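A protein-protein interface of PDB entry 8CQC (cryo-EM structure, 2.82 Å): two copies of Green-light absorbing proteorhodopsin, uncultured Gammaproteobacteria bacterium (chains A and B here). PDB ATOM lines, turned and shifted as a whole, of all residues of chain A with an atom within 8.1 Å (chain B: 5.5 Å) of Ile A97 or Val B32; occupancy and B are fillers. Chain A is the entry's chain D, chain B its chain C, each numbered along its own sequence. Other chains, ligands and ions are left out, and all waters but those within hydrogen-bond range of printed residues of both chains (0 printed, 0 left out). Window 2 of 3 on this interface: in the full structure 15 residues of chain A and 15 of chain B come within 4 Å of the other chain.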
ATOM      1  N   ILE A  72     -19.860   2.695 -12.651  1.00  0.00           N
ATOM      2  CA  ILE A  72     -20.553   1.856 -11.685  1.00  0.00           C
ATOM      3  C   ILE A  72     -20.253   2.383 -10.298  1.00  0.00           C
ATOM      4  O   ILE A  72     -21.162   2.579  -9.490  1.00  0.00           O
ATOM      5  CB  ILE A  72     -20.109   0.389 -11.778  1.00  0.00           C
ATOM      6  CG1 ILE A  72     -20.502  -0.203 -13.132  1.00  0.00           C
ATOM      7  CG2 ILE A  72     -20.720  -0.428 -10.650  1.00  0.00           C
ATOM      8  CD1 ILE A  72     -20.055  -1.635 -13.323  1.00  0.00           C
ATOM      9  N   HIS A  76     -23.165   3.398  -7.559  1.00  0.00           N
ATOM     10  CA  HIS A  76     -23.187   2.919  -6.177  1.00  0.00           C
ATOM     11  C   HIS A  76     -22.754   3.995  -5.109  1.00  0.00           C
ATOM     12  O   HIS A  76     -23.313   4.133  -3.982  1.00  0.00           O
ATOM     13  CB  HIS A  76     -22.298   1.685  -6.032  1.00  0.00           C
ATOM     14  CG  HIS A  76     -22.793   0.488  -6.781  1.00  0.00           C
ATOM     15  ND1 HIS A  76     -22.658   0.355  -8.145  1.00  0.00           N
ATOM     16  CD2 HIS A  76     -23.412  -0.638  -6.352  1.00  0.00           C
ATOM     17  CE1 HIS A  76     -23.180  -0.798  -8.527  1.00  0.00           C
ATOM     18  NE2 HIS A  76     -23.643  -1.420  -7.458  1.00  0.00           N
ATOM     19  N   PRO A  91     -21.867   1.048   4.316  1.00  0.00           N
ATOM     20  CA  PRO A  91     -22.557   0.442   3.179  1.00  0.00           C
ATOM     21  C   PRO A  91     -21.881  -0.852   2.765  1.00  0.00           C
ATOM     22  O   PRO A  91     -22.075  -1.298   1.640  1.00  0.00           O
ATOM     23  CB  PRO A  91     -22.388   1.491   2.085  1.00  0.00           C
ATOM     24  CG  PRO A  91     -21.123   2.215   2.439  1.00  0.00           C
ATOM     25  CD  PRO A  91     -20.792   1.954   3.884  1.00  0.00           C
ATOM     26  N   THR A  92     -21.115  -1.456   3.669  1.00  0.00           N
ATOM     27  CA  THR A  92     -20.410  -2.704   3.373  1.00  0.00           C
ATOM     28  C   THR A  92     -21.131  -3.591   2.366  1.00  0.00           C
ATOM     29  O   THR A  92     -20.547  -3.991   1.360  1.00  0.00           O
ATOM     30  CB  THR A  92     -20.184  -3.528   4.655  1.00  0.00           C
ATOM     31  OG1 THR A  92     -19.487  -2.734   5.622  1.00  0.00           O
ATOM     32  CG2 THR A  92     -19.374  -4.778   4.350  1.00  0.00           C
ATOM     33  N   VAL A  93     -22.392  -3.909   2.635  1.00  0.00           N
ATOM     34  CA  VAL A  93     -23.134  -4.794   1.745  1.00  0.00           C
ATOM     35  C   VAL A  93     -23.157  -4.227   0.339  1.00  0.00           C
ATOM     36  O   VAL A  93     -22.843  -4.927  -0.623  1.00  0.00           O
ATOM     37  CB  VAL A  93     -24.579  -4.999   2.230  1.00  0.00           C
ATOM     38  CG1 VAL A  93     -25.375  -5.793   1.207  1.00  0.00           C
ATOM     39  CG2 VAL A  93     -24.589  -5.692   3.582  1.00  0.00           C
ATOM     40  N   PHE A  94     -23.516  -2.956   0.215  1.00  0.00           N
ATOM     41  CA  PHE A  94     -23.517  -2.319  -1.090  1.00  0.00           C
ATOM     42  C   PHE A  94     -22.099  -2.280  -1.609  1.00  0.00           C
ATOM     43  O   PHE A  94     -21.869  -2.359  -2.815  1.00  0.00           O
ATOM     44  CB  PHE A  94     -24.069  -0.902  -0.994  1.00  0.00           C
ATOM     45  CG  PHE A  94     -25.295  -0.787  -0.137  1.00  0.00           C
ATOM     46  CD1 PHE A  94     -26.548  -1.066  -0.654  1.00  0.00           C
ATOM     47  CD2 PHE A  94     -25.193  -0.398   1.187  1.00  0.00           C
ATOM     48  CE1 PHE A  94     -27.677  -0.960   0.135  1.00  0.00           C
ATOM     49  CE2 PHE A  94     -26.318  -0.289   1.982  1.00  0.00           C
ATOM     50  CZ  PHE A  94     -27.561  -0.570   1.455  1.00  0.00           C
ATOM     51  N   ARG A  95     -21.109  -2.161  -0.691  1.00  0.00           N
ATOM     52  CA  ARG A  95     -19.745  -2.083  -1.100  1.00  0.00           C
ATOM     53  C   ARG A  95     -19.347  -3.438  -1.485  1.00  0.00           C
ATOM     54  O   ARG A  95     -18.336  -3.584  -2.038  1.00  0.00           O
ATOM     55  CB  ARG A  95     -18.868  -1.637   0.046  1.00  0.00           C
ATOM     56  CG  ARG A  95     -18.750  -0.142   0.205  1.00  0.00           C
ATOM     57  CD  ARG A  95     -17.412   0.226   0.795  1.00  0.00           C
ATOM     58  NE  ARG A  95     -17.411   1.582   1.315  1.00  0.00           N
ATOM     59  CZ  ARG A  95     -17.046   2.654   0.629  1.00  0.00           C
ATOM     60  NH1 ARG A  95     -16.643   2.542  -0.621  1.00  0.00           N
ATOM     61  NH2 ARG A  95     -17.080   3.837   1.204  1.00  0.00           N
ATOM     62  N   TYR A  96     -20.123  -4.489  -1.190  1.00  0.00           N
ATOM     63  CA  TYR A  96     -19.732  -5.790  -1.744  1.00  0.00           C
ATOM     64  C   TYR A  96     -20.377  -5.926  -3.100  1.00  0.00           C
ATOM     65  O   TYR A  96     -19.880  -6.643  -3.964  1.00  0.00           O
ATOM     66  CB  TYR A  96     -20.128  -6.937  -0.819  1.00  0.00           C
ATOM     67  CG  TYR A  96     -18.991  -7.407   0.058  1.00  0.00           C
ATOM     68  CD1 TYR A  96     -18.030  -8.280  -0.434  1.00  0.00           C
ATOM     69  CD2 TYR A  96     -18.871  -6.967   1.367  1.00  0.00           C
ATOM     70  CE1 TYR A  96     -16.982  -8.708   0.358  1.00  0.00           C
ATOM     71  CE2 TYR A  96     -17.826  -7.391   2.168  1.00  0.00           C
ATOM     72  CZ  TYR A  96     -16.886  -8.262   1.659  1.00  0.00           C
ATOM     73  OH  TYR A  96     -15.844  -8.685   2.450  1.00  0.00           O
ATOM     74  N   ILE A  97     -21.481  -5.229  -3.290  1.00  0.00           N
ATOM     75  CA  ILE A  97     -22.205  -5.234  -4.555  1.00  0.00           C
ATOM     76  C   ILE A  97     -21.382  -4.553  -5.634  1.00  0.00           C
ATOM     77  O   ILE A  97     -21.060  -5.161  -6.650  1.00  0.00           O
ATOM     78  CB  ILE A  97     -23.560  -4.518  -4.429  1.00  0.00           C
ATOM     79  CG1 ILE A  97     -24.434  -5.211  -3.383  1.00  0.00           C
ATOM     80  CG2 ILE A  97     -24.269  -4.481  -5.774  1.00  0.00           C
ATOM     81  CD1 ILE A  97     -25.739  -4.498  -3.109  1.00  0.00           C
ATOM     82  N   ASP A  98     -21.030  -3.287  -5.410  1.00  0.00           N
ATOM     83  CA  ASP A  98     -20.193  -2.589  -6.375  1.00  0.00           C
ATOM     84  C   ASP A  98     -18.908  -3.357  -6.614  1.00  0.00           C
ATOM     85  O   ASP A  98     -18.497  -3.547  -7.758  1.00  0.00           O
ATOM     86  CB  ASP A  98     -19.870  -1.178  -5.890  1.00  0.00           C
ATOM     87  CG  ASP A  98     -19.017  -0.406  -6.876  1.00  0.00           C
ATOM     88  OD1 ASP A  98     -17.785  -0.616  -6.892  1.00  0.00           O
ATOM     89  OD2 ASP A  98     -19.579   0.404  -7.641  1.00  0.00           O
ATOM     90  N   TRP A  99     -18.248  -3.775  -5.541  1.00  0.00           N
ATOM     91  CA  TRP A  99     -17.023  -4.544  -5.689  1.00  0.00           C
ATOM     92  C   TRP A  99     -17.298  -5.753  -6.561  1.00  0.00           C
ATOM     93  O   TRP A  99     -16.552  -6.033  -7.499  1.00  0.00           O
ATOM     94  CB  TRP A  99     -16.478  -4.970  -4.327  1.00  0.00           C
ATOM     95  CG  TRP A  99     -15.978  -3.822  -3.513  1.00  0.00           C
ATOM     96  CD1 TRP A  99     -15.876  -2.519  -3.909  1.00  0.00           C
ATOM     97  CD2 TRP A  99     -15.508  -3.867  -2.161  1.00  0.00           C
ATOM     98  NE1 TRP A  99     -15.372  -1.752  -2.888  1.00  0.00           N
ATOM     99  CE2 TRP A  99     -15.138  -2.556  -1.803  1.00  0.00           C
ATOM    100  CE3 TRP A  99     -15.365  -4.889  -1.219  1.00  0.00           C
ATOM    101  CZ2 TRP A  99     -14.635  -2.240  -0.544  1.00  0.00           C
ATOM    102  CZ3 TRP A  99     -14.864  -4.574   0.030  1.00  0.00           C
ATOM    103  CH2 TRP A  99     -14.505  -3.260   0.357  1.00  0.00           C
ATOM    104  N   LEU A 100     -18.377  -6.465  -6.262  1.00  0.00           N
ATOM    105  CA  LEU A 100     -18.744  -7.623  -7.063  1.00  0.00           C
ATOM    106  C   LEU A 100     -18.822  -7.248  -8.533  1.00  0.00           C
ATOM    107  O   LEU A 100     -18.492  -8.051  -9.403  1.00  0.00           O
ATOM    108  CB  LEU A 100     -20.084  -8.188  -6.598  1.00  0.00           C
ATOM    109  CG  LEU A 100     -20.568  -9.441  -7.327  1.00  0.00           C
ATOM    110  CD1 LEU A 100     -19.541 -10.554  -7.190  1.00  0.00           C
ATOM    111  CD2 LEU A 100     -21.918  -9.883  -6.787  1.00  0.00           C
ATOM    112  N   LEU A 101     -19.268  -6.039  -8.796  1.00  0.00           N
ATOM    113  CA  LEU A 101     -19.383  -5.582 -10.176  1.00  0.00           C
ATOM    114  C   LEU A 101     -18.089  -5.011 -10.747  1.00  0.00           C
ATOM    115  O   LEU A 101     -17.832  -5.179 -11.944  1.00  0.00           O
ATOM    116  CB  LEU A 101     -20.492  -4.539 -10.294  1.00  0.00           C
ATOM    117  CG  LEU A 101     -21.906  -5.109 -10.236  1.00  0.00           C
ATOM    118  CD1 LEU A 101     -22.912  -3.992 -10.176  1.00  0.00           C
ATOM    119  CD2 LEU A 101     -22.167  -5.999 -11.434  1.00  0.00           C
ATOM    120  N   THR A 102     -17.263  -4.346  -9.939  1.00  0.00           N
ATOM    121  CA  THR A 102     -16.114  -3.609 -10.458  1.00  0.00           C
ATOM    122  C   THR A 102     -14.797  -4.369 -10.371  1.00  0.00           C
ATOM    123  O   THR A 102     -13.963  -4.235 -11.268  1.00  0.00           O
ATOM    124  CB  THR A 102     -15.962  -2.271  -9.731  1.00  0.00           C
ATOM    125  OG1 THR A 102     -15.868  -2.498  -8.321  1.00  0.00           O
ATOM    126  CG2 THR A 102     -17.146  -1.368 -10.018  1.00  0.00           C
ATOM    127  N   VAL A 103     -14.569  -5.139  -9.303  1.00  0.00           N
ATOM    128  CA  VAL A 103     -13.317  -5.891  -9.183  1.00  0.00           C
ATOM    129  C   VAL A 103     -13.113  -6.852 -10.344  1.00  0.00           C
ATOM    130  O   VAL A 103     -11.980  -6.951 -10.842  1.00  0.00           O
ATOM    131  CB  VAL A 103     -13.242  -6.576  -7.812  1.00  0.00           C
ATOM    132  CG1 VAL A 103     -11.978  -7.402  -7.692  1.00  0.00           C
ATOM    133  CG2 VAL A 103     -13.306  -5.546  -6.707  1.00  0.00           C
ATOM    134  N   PRO A 104     -14.118  -7.606 -10.812  1.00  0.00           N
ATOM    135  CA  PRO A 104     -13.890  -8.422 -12.015  1.00  0.00           C
ATOM    136  C   PRO A 104     -13.434  -7.617 -13.218  1.00  0.00           C
ATOM    137  O   PRO A 104     -12.518  -8.049 -13.922  1.00  0.00           O
ATOM    138  CB  PRO A 104     -15.257  -9.073 -12.248  1.00  0.00           C
ATOM    139  CG  PRO A 104     -15.843  -9.167 -10.903  1.00  0.00           C
ATOM    140  CD  PRO A 104     -15.420  -7.920 -10.195  1.00  0.00           C
ATOM    141  N   LEU A 136     -14.108 -12.258  -3.376  1.00  0.00           N
ATOM    142  CA  LEU A 136     -15.205 -11.407  -2.922  1.00  0.00           C
ATOM    143  C   LEU A 136     -16.275 -12.208  -2.190  1.00  0.00           C
ATOM    144  O   LEU A 136     -16.808 -11.754  -1.169  1.00  0.00           O
ATOM    145  CB  LEU A 136     -15.812 -10.657  -4.106  1.00  0.00           C
ATOM    146  CG  LEU A 136     -14.935  -9.559  -4.705  1.00  0.00           C
ATOM    147  CD1 LEU A 136     -15.533  -9.059  -6.002  1.00  0.00           C
ATOM    148  CD2 LEU A 136     -14.761  -8.421  -3.719  1.00  0.00           C
ATOM    149  N   TYR A 140     -17.384 -11.652   1.694  1.00  0.00           N
ATOM    150  CA  TYR A 140     -18.741 -11.350   2.140  1.00  0.00           C
ATOM    151  C   TYR A 140     -19.246 -12.387   3.133  1.00  0.00           C
ATOM    152  O   TYR A 140     -19.946 -12.042   4.092  1.00  0.00           O
ATOM    153  CB  TYR A 140     -19.699 -11.254   0.956  1.00  0.00           C
ATOM    154  CG  TYR A 140     -21.133 -11.111   1.405  1.00  0.00           C
ATOM    155  CD1 TYR A 140     -21.584  -9.931   1.978  1.00  0.00           C
ATOM    156  CD2 TYR A 140     -22.031 -12.162   1.278  1.00  0.00           C
ATOM    157  CE1 TYR A 140     -22.889  -9.796   2.402  1.00  0.00           C
ATOM    158  CE2 TYR A 140     -23.340 -12.036   1.700  1.00  0.00           C
ATOM    159  CZ  TYR A 140     -23.763 -10.852   2.260  1.00  0.00           C
ATOM    160  OH  TYR A 140     -25.066 -10.720   2.682  1.00  0.00           O
ATOM    161  N   ASP B  25     -32.489  -5.889   3.749  1.00  0.00           N
ATOM    162  CA  ASP B  25     -31.466  -6.359   4.675  1.00  0.00           C
ATOM    163  C   ASP B  25     -30.424  -7.217   3.962  1.00  0.00           C
ATOM    164  O   ASP B  25     -30.161  -7.036   2.773  1.00  0.00           O
ATOM    165  CB  ASP B  25     -32.103  -7.148   5.822  1.00  0.00           C
ATOM    166  CG  ASP B  25     -32.998  -8.276   5.334  1.00  0.00           C
ATOM    167  OD1 ASP B  25     -33.199  -8.396   4.107  1.00  0.00           O
ATOM    168  OD2 ASP B  25     -33.502  -9.043   6.181  1.00  0.00           O
ATOM    169  N   ASP B  28     -32.929 -11.050   2.536  1.00  0.00           N
ATOM    170  CA  ASP B  28     -33.934 -11.149   1.484  1.00  0.00           C
ATOM    171  C   ASP B  28     -33.329 -11.672   0.187  1.00  0.00           C
ATOM    172  O   ASP B  28     -33.939 -12.502  -0.499  1.00  0.00           O
ATOM    173  CB  ASP B  28     -34.600  -9.792   1.259  1.00  0.00           C
ATOM    174  CG  ASP B  28     -33.601  -8.691   0.955  1.00  0.00           C
ATOM    175  OD1 ASP B  28     -32.383  -8.937   1.078  1.00  0.00           O
ATOM    176  OD2 ASP B  28     -34.036  -7.579   0.591  1.00  0.00           O
ATOM    177  N   TYR B  29     -32.133 -11.196  -0.165  1.00  0.00           N
ATOM    178  CA  TYR B  29     -31.416 -11.594  -1.375  1.00  0.00           C
ATOM    179  C   TYR B  29     -32.218 -11.334  -2.645  1.00  0.00           C
ATOM    180  O   TYR B  29     -31.906 -11.888  -3.702  1.00  0.00           O
ATOM    181  CB  TYR B  29     -30.992 -13.066  -1.310  1.00  0.00           C
ATOM    182  CG  TYR B  29     -29.931 -13.345  -0.271  1.00  0.00           C
ATOM    183  CD1 TYR B  29     -28.865 -12.473  -0.088  1.00  0.00           C
ATOM    184  CD2 TYR B  29     -29.999 -14.474   0.534  1.00  0.00           C
ATOM    185  CE1 TYR B  29     -27.895 -12.721   0.862  1.00  0.00           C
ATOM    186  CE2 TYR B  29     -29.033 -14.730   1.487  1.00  0.00           C
ATOM    187  CZ  TYR B  29     -27.984 -13.850   1.647  1.00  0.00           C
ATOM    188  OH  TYR B  29     -27.022 -14.103   2.596  1.00  0.00           O
ATOM    189  N   THR B  30     -33.279 -10.501  -2.549  1.00  0.00           N
ATOM    190  CA  THR B  30     -34.092 -10.169  -3.712  1.00  0.00           C
ATOM    191  C   THR B  30     -33.839  -8.733  -4.134  1.00  0.00           C
ATOM    192  O   THR B  30     -33.516  -8.469  -5.290  1.00  0.00           O
ATOM    193  CB  THR B  30     -35.592 -10.359  -3.430  1.00  0.00           C
ATOM    194  OG1 THR B  30     -35.834 -11.708  -3.013  1.00  0.00           O
ATOM    195  CG2 THR B  30     -36.409 -10.063  -4.678  1.00  0.00           C
ATOM    196  N   GLY B  31     -33.985  -7.800  -3.200  1.00  0.00           N
ATOM    197  CA  GLY B  31     -33.709  -6.410  -3.507  1.00  0.00           C
ATOM    198  C   GLY B  31     -32.258  -6.261  -3.908  1.00  0.00           C
ATOM    199  O   GLY B  31     -31.931  -5.487  -4.807  1.00  0.00           O
ATOM    200  N   VAL B  32     -31.380  -7.005  -3.244  1.00  0.00           N
ATOM    201  CA  VAL B  32     -29.965  -6.951  -3.573  1.00  0.00           C
ATOM    202  C   VAL B  32     -29.752  -7.383  -5.012  1.00  0.00           C
ATOM    203  O   VAL B  32     -29.077  -6.696  -5.779  1.00  0.00           O
ATOM    204  CB  VAL B  32     -29.140  -7.865  -2.655  1.00  0.00           C
ATOM    205  CG1 VAL B  32     -27.659  -7.734  -2.970  1.00  0.00           C
ATOM    206  CG2 VAL B  32     -29.416  -7.537  -1.195  1.00  0.00           C
ATOM    207  N   SER B  33     -30.336  -8.516  -5.385  1.00  0.00           N
ATOM    208  CA  SER B  33     -30.215  -8.985  -6.757  1.00  0.00           C
ATOM    209  C   SER B  33     -30.729  -7.899  -7.677  1.00  0.00           C
ATOM    210  O   SER B  33     -30.111  -7.595  -8.700  1.00  0.00           O
ATOM    211  CB  SER B  33     -30.997 -10.282  -6.968  1.00  0.00           C
ATOM    212  OG  SER B  33     -32.391 -10.071  -6.840  1.00  0.00           O
ATOM    213  N   PHE B  34     -31.856  -7.299  -7.314  1.00  0.00           N
ATOM    214  CA  PHE B  34     -32.415  -6.217  -8.118  1.00  0.00           C
ATOM    215  C   PHE B  34     -31.367  -5.149  -8.395  1.00  0.00           C
ATOM    216  O   PHE B  34     -31.177  -4.734  -9.543  1.00  0.00           O
ATOM    217  CB  PHE B  34     -33.629  -5.608  -7.417  1.00  0.00           C
ATOM    218  CG  PHE B  34     -34.948  -6.113  -7.932  1.00  0.00           C
ATOM    219  CD1 PHE B  34     -35.484  -5.612  -9.107  1.00  0.00           C
ATOM    220  CD2 PHE B  34     -35.659  -7.077  -7.236  1.00  0.00           C
ATOM    221  CE1 PHE B  34     -36.699  -6.071  -9.582  1.00  0.00           C
ATOM    222  CE2 PHE B  34     -36.874  -7.538  -7.704  1.00  0.00           C
ATOM    223  CZ  PHE B  34     -37.394  -7.035  -8.878  1.00  0.00           C
ATOM    224  N   TRP B  35     -30.666  -4.698  -7.352  1.00  0.00           N
ATOM    225  CA  TRP B  35     -29.638  -3.677  -7.539  1.00  0.00           C
ATOM    226  C   TRP B  35     -28.496  -4.190  -8.406  1.00  0.00           C
ATOM    227  O   TRP B  35     -28.012  -3.478  -9.299  1.00  0.00           O
ATOM    228  CB  TRP B  35     -29.114  -3.201  -6.185  1.00  0.00           C
ATOM    229  CG  TRP B  35     -30.096  -2.359  -5.439  1.00  0.00           C
ATOM    230  CD1 TRP B  35     -30.718  -2.668  -4.267  1.00  0.00           C
ATOM    231  CD2 TRP B  35     -30.584  -1.070  -5.823  1.00  0.00           C
ATOM    232  NE1 TRP B  35     -31.560  -1.650  -3.895  1.00  0.00           N
ATOM    233  CE2 TRP B  35     -31.495  -0.656  -4.835  1.00  0.00           C
ATOM    234  CE3 TRP B  35     -30.337  -0.223  -6.909  1.00  0.00           C
ATOM    235  CZ2 TRP B  35     -32.159   0.566  -4.895  1.00  0.00           C
ATOM    236  CZ3 TRP B  35     -30.995   0.987  -6.969  1.00  0.00           C
ATOM    237  CH2 TRP B  35     -31.895   1.371  -5.967  1.00  0.00           C
ATOM    238  N   LEU B  36     -28.059  -5.428  -8.166  1.00  0.00           N
ATOM    239  CA  LEU B  36     -26.960  -5.996  -8.936  1.00  0.00           C
ATOM    240  C   LEU B  36     -27.307  -6.072 -10.417  1.00  0.00           C
ATOM    241  O   LEU B  36     -26.537  -5.622 -11.274  1.00  0.00           O
ATOM    242  CB  LEU B  36     -26.622  -7.382  -8.385  1.00  0.00           C
ATOM    243  CG  LEU B  36     -25.280  -8.014  -8.736  1.00  0.00           C
ATOM    244  CD1 LEU B  36     -24.154  -7.280  -8.038  1.00  0.00           C
ATOM    245  CD2 LEU B  36     -25.284  -9.481  -8.353  1.00  0.00           C
ATOM    246  N   VAL B  37     -28.482  -6.618 -10.736  1.00  0.00           N
ATOM    247  CA  VAL B  37     -28.896  -6.775 -12.125  1.00  0.00           C
ATOM    248  C   VAL B  37     -29.148  -5.419 -12.768  1.00  0.00           C
ATOM    249  O   VAL B  37     -28.848  -5.220 -13.946  1.00  0.00           O
ATOM    250  CB  VAL B  37     -30.132  -7.687 -12.213  1.00  0.00           C
ATOM    251  CG1 VAL B  37     -30.658  -7.740 -13.631  1.00  0.00           C
ATOM    252  CG2 VAL B  37     -29.787  -9.085 -11.737  1.00  0.00           C
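The side-chain hydroxyl (OH) of Tyr A96 sits close to the backbone NH (N) of Tyr A140 (3.4 Å).
CD1 of Ile A97 touches CG1 of Val B32, at 3.8 Å.
Leu B36 touches Ile A97.
Leu A100 touches Leu B36 (CD2 to CD1, 3.7 Å).
Leu A101 touches Leu B36 (CG to CD1, 3.8 Å).
Tyr A140 touches Tyr B29.
Ile A97 touches just these residues of chain B: Val B32 (3.8 Å) and Leu B36 (3.6 Å).
Of chain A, only Ile A97 comes within 4 Å of Val B32.
No residue of chain A comes within 4 Å of Gly B31.
Of the printed residues of chain A, Tyr B29 touches Tyr A140 (3.9 Å).
Of the printed residues of chain B, Tyr A140 touches Tyr B29 (3.9 Å).
Of the printed residues of chain B, Leu A100 touches Leu B36.
Of the printed residues of chain A, Leu B36 touches Ile A97, Leu A100 and Leu A101.
Printed residues of chain B within 4 Å of Leu A101: Leu B36 (3.8 Å).
Tyr A96 touches none of the printed residues of chain B.
The nearest residue of chain A that does not touch Val B32 is Val A93 (5.0 Å).
Of the 11 printed residues of chain B, 3 touch a printed residue of chain A.
Among the printed residues, 5 pairs touch across the chains.
Among the printed residues, no Asp or Glu carboxylate lies within 4 Å of a Lys or Arg side-chain nitrogen of the other chain.
No position is printed for both chains.
Of the 5 pairs that touch across the chains among the printed residues, none has its exchanged pair printed and touching as well.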
